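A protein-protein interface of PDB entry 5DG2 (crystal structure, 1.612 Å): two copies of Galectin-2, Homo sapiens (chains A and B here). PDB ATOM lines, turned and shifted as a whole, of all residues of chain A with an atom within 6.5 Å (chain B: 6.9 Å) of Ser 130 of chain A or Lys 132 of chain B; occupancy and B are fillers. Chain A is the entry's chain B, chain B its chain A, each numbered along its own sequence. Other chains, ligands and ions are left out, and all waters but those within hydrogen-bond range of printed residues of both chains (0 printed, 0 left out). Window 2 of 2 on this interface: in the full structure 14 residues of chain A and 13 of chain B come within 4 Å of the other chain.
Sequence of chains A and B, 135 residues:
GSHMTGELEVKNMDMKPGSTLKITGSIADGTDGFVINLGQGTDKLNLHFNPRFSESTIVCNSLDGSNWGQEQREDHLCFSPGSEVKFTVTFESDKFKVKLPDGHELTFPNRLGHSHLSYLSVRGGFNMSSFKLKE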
ATOM      1  N   LYS A  22       1.472   8.395  13.405  1.00  0.00           N
ATOM      2  CA  LYS A  22       0.697   7.320  12.804  1.00  0.00           C
ATOM      3  C   LYS A  22       1.044   6.017  13.483  1.00  0.00           C
ATOM      4  O   LYS A  22       2.216   5.677  13.641  1.00  0.00           O
ATOM      5  CB  LYS A  22       0.950   7.226  11.298  1.00  0.00           C
ATOM      6  CG  LYS A  22       0.558   8.486  10.537  1.00  0.00           C
ATOM      7  CD  LYS A  22       0.835   8.340   9.045  1.00  0.00           C
ATOM      8  CE  LYS A  22       0.251   9.504   8.250  1.00  0.00           C
ATOM      9  NZ  LYS A  22      -1.238   9.464   8.184  1.00  0.00           N
ATOM     10  N   ILE A  23       0.016   5.276  13.871  1.00  0.00           N
ATOM     11  CA  ILE A  23       0.203   4.070  14.640  1.00  0.00           C
ATOM     12  C   ILE A  23      -0.511   2.913  13.959  1.00  0.00           C
ATOM     13  O   ILE A  23      -1.666   3.057  13.566  1.00  0.00           O
ATOM     14  CB  ILE A  23      -0.356   4.236  16.049  1.00  0.00           C
ATOM     15  CG1 ILE A  23       0.556   5.126  16.889  1.00  0.00           C
ATOM     16  CG2 ILE A  23      -0.574   2.884  16.696  1.00  0.00           C
ATOM     17  CD1 ILE A  23      -0.098   5.575  18.178  1.00  0.00           C
ATOM     18  N   THR A  24       0.175   1.784  13.790  1.00  0.00           N
ATOM     19  CA  THR A  24      -0.488   0.586  13.273  1.00  0.00           C
ATOM     20  C   THR A  24      -0.363  -0.520  14.295  1.00  0.00           C
ATOM     21  O   THR A  24       0.650  -0.634  14.983  1.00  0.00           O
ATOM     22  CB  THR A  24       0.115   0.120  11.928  1.00  0.00           C
ATOM     23  OG1 THR A  24       0.004   1.175  10.967  1.00  0.00           O
ATOM     24  CG2 THR A  24      -0.617  -1.116  11.400  1.00  0.00           C
ATOM     25  N   GLY A  25      -1.397  -1.343  14.411  1.00  0.00           N
ATOM     26  CA  GLY A  25      -1.301  -2.481  15.288  1.00  0.00           C
ATOM     27  C   GLY A  25      -2.402  -3.495  15.058  1.00  0.00           C
ATOM     28  O   GLY A  25      -3.303  -3.297  14.233  1.00  0.00           O
ATOM     29  N   LYS A  86      -5.326   1.158  11.981  1.00  0.00           N
ATOM     30  CA  LYS A  86      -4.394   2.255  11.855  1.00  0.00           C
ATOM     31  C   LYS A  86      -5.070   3.485  12.451  1.00  0.00           C
ATOM     32  O   LYS A  86      -6.271   3.689  12.259  1.00  0.00           O
ATOM     33  CB  LYS A  86      -4.011   2.488  10.394  1.00  0.00           C
ATOM     34  CG  LYS A  86      -3.368   1.273   9.723  1.00  0.00           C
ATOM     35  CD  LYS A  86      -3.106   1.524   8.248  1.00  0.00           C
ATOM     36  CE  LYS A  86      -2.349   0.364   7.624  1.00  0.00           C
ATOM     37  NZ  LYS A  86      -1.005   0.222   8.241  1.00  0.00           N
ATOM     38  N   ASN A 127      -1.359  -4.839  20.001  1.00  0.00           N
ATOM     39  CA  ASN A 127       0.029  -5.058  19.642  1.00  0.00           C
ATOM     40  C   ASN A 127       0.468  -4.026  18.623  1.00  0.00           C
ATOM     41  O   ASN A 127       0.107  -4.121  17.458  1.00  0.00           O
ATOM     42  CB  ASN A 127       0.226  -6.461  19.074  1.00  0.00           C
ATOM     43  CG  ASN A 127       1.611  -6.650  18.489  1.00  0.00           C
ATOM     44  OD1 ASN A 127       2.587  -6.787  19.223  1.00  0.00           O
ATOM     45  ND2 ASN A 127       1.703  -6.664  17.160  1.00  0.00           N
ATOM     46  N   MET A 128       1.233  -3.033  19.057  1.00  0.00           N
ATOM     47  CA  MET A 128       1.642  -1.973  18.142  1.00  0.00           C
ATOM     48  C   MET A 128       2.783  -2.473  17.277  1.00  0.00           C
ATOM     49  O   MET A 128       3.832  -2.853  17.787  1.00  0.00           O
ATOM     50  CB  MET A 128       2.062  -0.717  18.908  1.00  0.00           C
ATOM     51  CG  MET A 128       2.379   0.454  18.001  1.00  0.00           C
ATOM     52  SD  MET A 128       2.721   1.974  18.927  1.00  0.00           S
ATOM     53  CE  MET A 128       1.120   2.442  19.541  1.00  0.00           C
ATOM     54  N   SER A 129       2.570  -2.479  15.966  1.00  0.00           N
ATOM     55  CA  SER A 129       3.571  -2.998  15.049  1.00  0.00           C
ATOM     56  C   SER A 129       4.344  -1.878  14.355  1.00  0.00           C
ATOM     57  O   SER A 129       5.428  -2.109  13.825  1.00  0.00           O
ATOM     58  CB  SER A 129       2.919  -3.914  14.014  1.00  0.00           C
ATOM     59  OG  SER A 129       1.989  -3.219  13.210  1.00  0.00           O
ATOM     60  N   SER A 130       3.800  -0.671  14.335  1.00  0.00           N
ATOM     61  CA  SER A 130       4.577   0.433  13.791  1.00  0.00           C
ATOM     62  C   SER A 130       4.115   1.771  14.296  1.00  0.00           C
ATOM     63  O   SER A 130       2.951   1.958  14.640  1.00  0.00           O
ATOM     64  CB  SER A 130       4.545   0.422  12.257  1.00  0.00           C
ATOM     65  OG  SER A 130       3.380   1.032  11.749  1.00  0.00           O
ATOM     66  N   PHE A 131       5.052   2.702  14.366  1.00  0.00           N
ATOM     67  CA  PHE A 131       4.668   4.082  14.553  1.00  0.00           C
ATOM     68  C   PHE A 131       5.567   4.983  13.734  1.00  0.00           C
ATOM     69  O   PHE A 131       6.721   4.658  13.416  1.00  0.00           O
ATOM     70  CB  PHE A 131       4.644   4.484  16.037  1.00  0.00           C
ATOM     71  CG  PHE A 131       5.978   4.450  16.719  1.00  0.00           C
ATOM     72  CD1 PHE A 131       6.357   3.341  17.460  1.00  0.00           C
ATOM     73  CD2 PHE A 131       6.826   5.545  16.668  1.00  0.00           C
ATOM     74  CE1 PHE A 131       7.586   3.310  18.112  1.00  0.00           C
ATOM     75  CE2 PHE A 131       8.048   5.527  17.312  1.00  0.00           C
ATOM     76  CZ  PHE A 131       8.431   4.402  18.036  1.00  0.00           C
ATOM     77  N   LYS A 132       4.990   6.103  13.342  1.00  0.00           N
ATOM     78  CA  LYS A 132       5.645   7.021  12.445  1.00  0.00           C
ATOM     79  C   LYS A 132       5.341   8.425  12.882  1.00  0.00           C
ATOM     80  O   LYS A 132       4.177   8.818  12.957  1.00  0.00           O
ATOM     81  CB  LYS A 132       5.184   6.791  11.004  1.00  0.00           C
ATOM     82  CG  LYS A 132       5.817   7.738  10.005  1.00  0.00           C
ATOM     83  CD  LYS A 132       5.179   7.611   8.637  1.00  0.00           C
ATOM     84  CE  LYS A 132       5.306   6.198   8.094  1.00  0.00           C
ATOM     85  NZ  LYS A 132       4.557   6.030   6.815  1.00  0.00           N
ATOM     86  N   THR B  20      11.806  -8.916  12.254  1.00  0.00           N
ATOM     87  CA  THR B  20      12.564  -7.855  11.621  1.00  0.00           C
ATOM     88  C   THR B  20      12.141  -6.508  12.205  1.00  0.00           C
ATOM     89  O   THR B  20      10.970  -6.290  12.481  1.00  0.00           O
ATOM     90  CB  THR B  20      12.371  -7.889  10.086  1.00  0.00           C
ATOM     91  OG1 THR B  20      13.211  -8.907   9.524  1.00  0.00           O
ATOM     92  CG2 THR B  20      12.722  -6.570   9.451  1.00  0.00           C
ATOM     93  N   LEU B  21      13.106  -5.625  12.399  1.00  0.00           N
ATOM     94  CA  LEU B  21      12.825  -4.297  12.910  1.00  0.00           C
ATOM     95  C   LEU B  21      13.351  -3.281  11.911  1.00  0.00           C
ATOM     96  O   LEU B  21      14.527  -3.294  11.567  1.00  0.00           O
ATOM     97  CB  LEU B  21      13.474  -4.105  14.277  1.00  0.00           C
ATOM     98  CG  LEU B  21      13.462  -2.689  14.828  1.00  0.00           C
ATOM     99  CD1 LEU B  21      12.018  -2.272  15.138  1.00  0.00           C
ATOM    100  CD2 LEU B  21      14.364  -2.597  16.051  1.00  0.00           C
ATOM    101  N   LYS B  22      12.474  -2.418  11.427  1.00  0.00           N
ATOM    102  CA  LYS B  22      12.861  -1.389  10.475  1.00  0.00           C
ATOM    103  C   LYS B  22      12.831  -0.045  11.156  1.00  0.00           C
ATOM    104  O   LYS B  22      11.842   0.333  11.776  1.00  0.00           O
ATOM    105  CB  LYS B  22      11.949  -1.388   9.248  1.00  0.00           C
ATOM    106  CG  LYS B  22      11.987  -2.670   8.444  1.00  0.00           C
ATOM    107  CD  LYS B  22      11.106  -2.555   7.199  1.00  0.00           C
ATOM    108  CE  LYS B  22      11.164  -3.825   6.356  1.00  0.00           C
ATOM    109  NZ  LYS B  22      10.561  -3.634   5.004  1.00  0.00           N
ATOM    110  N   ILE B  23      13.936   0.670  11.043  1.00  0.00           N
ATOM    111  CA  ILE B  23      14.078   1.957  11.693  1.00  0.00           C
ATOM    112  C   ILE B  23      14.413   3.019  10.664  1.00  0.00           C
ATOM    113  O   ILE B  23      15.328   2.837   9.861  1.00  0.00           O
ATOM    114  CB  ILE B  23      15.192   1.927  12.755  1.00  0.00           C
ATOM    115  CG1 ILE B  23      14.810   0.989  13.892  1.00  0.00           C
ATOM    116  CG2 ILE B  23      15.490   3.325  13.260  1.00  0.00           C
ATOM    117  CD1 ILE B  23      15.995   0.401  14.605  1.00  0.00           C
ATOM    118  N   THR B  24      13.672   4.121  10.692  1.00  0.00           N
ATOM    119  CA  THR B  24      13.914   5.240   9.799  1.00  0.00           C
ATOM    120  C   THR B  24      14.246   6.456  10.649  1.00  0.00           C
ATOM    121  O   THR B  24      13.661   6.646  11.719  1.00  0.00           O
ATOM    122  CB  THR B  24      12.687   5.521   8.901  1.00  0.00           C
ATOM    123  OG1 THR B  24      12.447   4.388   8.050  1.00  0.00           O
ATOM    124  CG2 THR B  24      12.905   6.748   8.044  1.00  0.00           C
ATOM    125  N   MET B 128      15.033   9.405  15.346  1.00  0.00           N
ATOM    126  CA  MET B 128      14.202   8.334  14.800  1.00  0.00           C
ATOM    127  C   MET B 128      12.791   8.807  14.527  1.00  0.00           C
ATOM    128  O   MET B 128      12.111   9.310  15.431  1.00  0.00           O
ATOM    129  CB  MET B 128      14.131   7.132  15.725  1.00  0.00           C
ATOM    130  CG  MET B 128      13.339   6.009  15.064  1.00  0.00           C
ATOM    131  SD  MET B 128      12.744   4.744  16.179  1.00  0.00           S
ATOM    132  CE  MET B 128      14.279   3.985  16.586  1.00  0.00           C
ATOM    133  N   SER B 130      10.562   6.686  12.536  1.00  0.00           N
ATOM    134  CA  SER B 130       9.679   5.552  12.268  1.00  0.00           C
ATOM    135  C   SER B 130      10.261   4.251  12.783  1.00  0.00           C
ATOM    136  O   SER B 130      11.468   4.029  12.731  1.00  0.00           O
ATOM    137  CB  SER B 130       9.400   5.432  10.768  1.00  0.00           C
ATOM    138  OG  SER B 130       8.599   4.297  10.493  1.00  0.00           O
ATOM    139  N   PHE B 131       9.368   3.385  13.247  1.00  0.00           N
ATOM    140  CA  PHE B 131       9.702   2.117  13.883  1.00  0.00           C
ATOM    141  C   PHE B 131       8.699   1.105  13.325  1.00  0.00           C
ATOM    142  O   PHE B 131       7.509   1.391  13.318  1.00  0.00           O
ATOM    143  CB  PHE B 131       9.600   2.299  15.415  1.00  0.00           C
ATOM    144  CG  PHE B 131       9.496   1.027  16.217  1.00  0.00           C
ATOM    145  CD1 PHE B 131       8.283   0.368  16.362  1.00  0.00           C
ATOM    146  CD2 PHE B 131      10.593   0.549  16.912  1.00  0.00           C
ATOM    147  CE1 PHE B 131       8.185  -0.787  17.123  1.00  0.00           C
ATOM    148  CE2 PHE B 131      10.502  -0.604  17.685  1.00  0.00           C
ATOM    149  CZ  PHE B 131       9.301  -1.275  17.789  1.00  0.00           C
ATOM    150  N   LYS B 132       9.160  -0.037  12.816  1.00  0.00           N
ATOM    151  CA  LYS B 132       8.239  -1.071  12.343  1.00  0.00           C
ATOM    152  C   LYS B 132       8.742  -2.467  12.682  1.00  0.00           C
ATOM    153  O   LYS B 132       9.837  -2.853  12.273  1.00  0.00           O
ATOM    154  CB  LYS B 132       8.011  -0.970  10.832  1.00  0.00           C
ATOM    155  CG  LYS B 132       7.053  -2.041  10.312  1.00  0.00           C
ATOM    156  CD  LYS B 132       6.314  -1.599   9.064  1.00  0.00           C
ATOM    157  CE  LYS B 132       7.207  -1.637   7.842  1.00  0.00           C
ATOM    158  NZ  LYS B 132       6.448  -1.283   6.607  1.00  0.00           N
ATOM    159  N   LEU B 133       7.936  -3.219  13.408  1.00  0.00           N
ATOM    160  CA  LEU B 133       8.299  -4.560  13.815  1.00  0.00           C
ATOM    161  C   LEU B 133       7.464  -5.591  13.050  1.00  0.00           C
ATOM    162  O   LEU B 133       6.266  -5.445  12.949  1.00  0.00           O
ATOM    163  CB  LEU B 133       8.085  -4.709  15.317  1.00  0.00           C
ATOM    164  CG  LEU B 133       8.738  -5.884  16.033  1.00  0.00           C
ATOM    165  CD1 LEU B 133      10.070  -6.311  15.435  1.00  0.00           C
ATOM    166  CD2 LEU B 133       8.864  -5.611  17.517  1.00  0.00           C
ATOM    167  N   LYS B 134       8.111  -6.611  12.496  1.00  0.00           N
ATOM    168  CA  LYS B 134       7.397  -7.664  11.777  1.00  0.00           C
ATOM    169  C   LYS B 134       7.825  -9.021  12.298  1.00  0.00           C
ATOM    170  O   LYS B 134       9.020  -9.300  12.376  1.00  0.00           O
ATOM    171  CB  LYS B 134       7.641  -7.580  10.267  1.00  0.00           C
ATOM    172  CG  LYS B 134       7.770  -6.168   9.728  1.00  0.00           C
ATOM    173  CD  LYS B 134       7.648  -6.126   8.209  1.00  0.00           C
ATOM    174  CE  LYS B 134       6.249  -5.669   7.789  1.00  0.00           C
ATOM    175  NZ  LYS B 134       6.254  -4.879   6.524  1.00  0.00           N
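N of Phe 131 of chain B sits at hydrogen-bond distance from O of Phe 131 of chain A (2.9 Å). The side-chain hydroxyl (OG) of Ser 130 of chain B sits close to the backbone carbonyl oxygen (O) of Phe 131 of chain A, at 3.5 Å. The backbone NH (N) of Leu 133 of chain B sits at hydrogen-bond distance from the backbone carbonyl oxygen (O) of Ser 129 of chain A.
The backbone NH of Ser 129 of chain A is in hydrogen-bond range of the backbone carbonyl oxygen of Thr 24 of chain A (2.8 Å). The backbone NH (N) of Lys 22 of chain B sits at hydrogen-bond distance from the backbone carbonyl oxygen (O) of Lys 132 of chain B, 2.8 Å away. The backbone NH (N) of Thr 24 of chain B sits at hydrogen-bond distance from the backbone carbonyl oxygen (O) of Ser 130 of chain B, at 3.0 Å. The backbone NH of Thr 24 of chain A sits at hydrogen-bond distance from the backbone carbonyl oxygen of Ser 130 of chain A (2.9 Å).
Among the printed residues, merely in contact across the chains: Ser 130 of chain A with Phe 131 of chain B (3.1 Å), Ser 129 of chain A with Lys 132 of chain B (3.3 Å) and Ser 130 of chain A with Lys 132 of chain B (3.99 Å).
Of the printed residues of chain A, Lys 132 of chain B touches Ser 129 and Ser 130. Of the printed residues of chain B, Phe 131 of chain A touches Ser 130 and Phe 131. Printed residues of chain A within 4 Å of Ser 130 of chain B: Phe 131 (3.3 Å). Of the printed residues of chain A, Leu 133 of chain B touches Ser 129. Printed residues of chain A within 4 Å of Phe 131 of chain B: Ser 130 (3.1 Å) and Phe 131 (2.9 Å). Printed residues of chain B within 4 Å of Ser 129 of chain A: Lys 132 and Leu 133. The nearest printed residue of chain A that does not touch Lys 132 of chain B is Phe 131 of chain A (5.2 Å).
Of the 11 printed residues of chain A, 3 touch a printed residue of chain B. Of the 11 printed residues of chain B, 4 touch a printed residue of chain A. Among the printed residues, no Asp or Glu carboxylate lies within 4 Å of a Lys or Arg side-chain nitrogen of the other chain.
Ser 130 of chain A touches Phe 131 of chain B, and with the chains exchanged Phe 131 of chain A touches Ser 130 of chain B. Ser 130 of chain A touches Lys 132 of chain B, but with the chains exchanged Lys 132 of chain A does not touch Ser 130 of chain B (4.3 Å). Phe 131 of chain A touches its own counterpart, Phe 131 of chain B.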
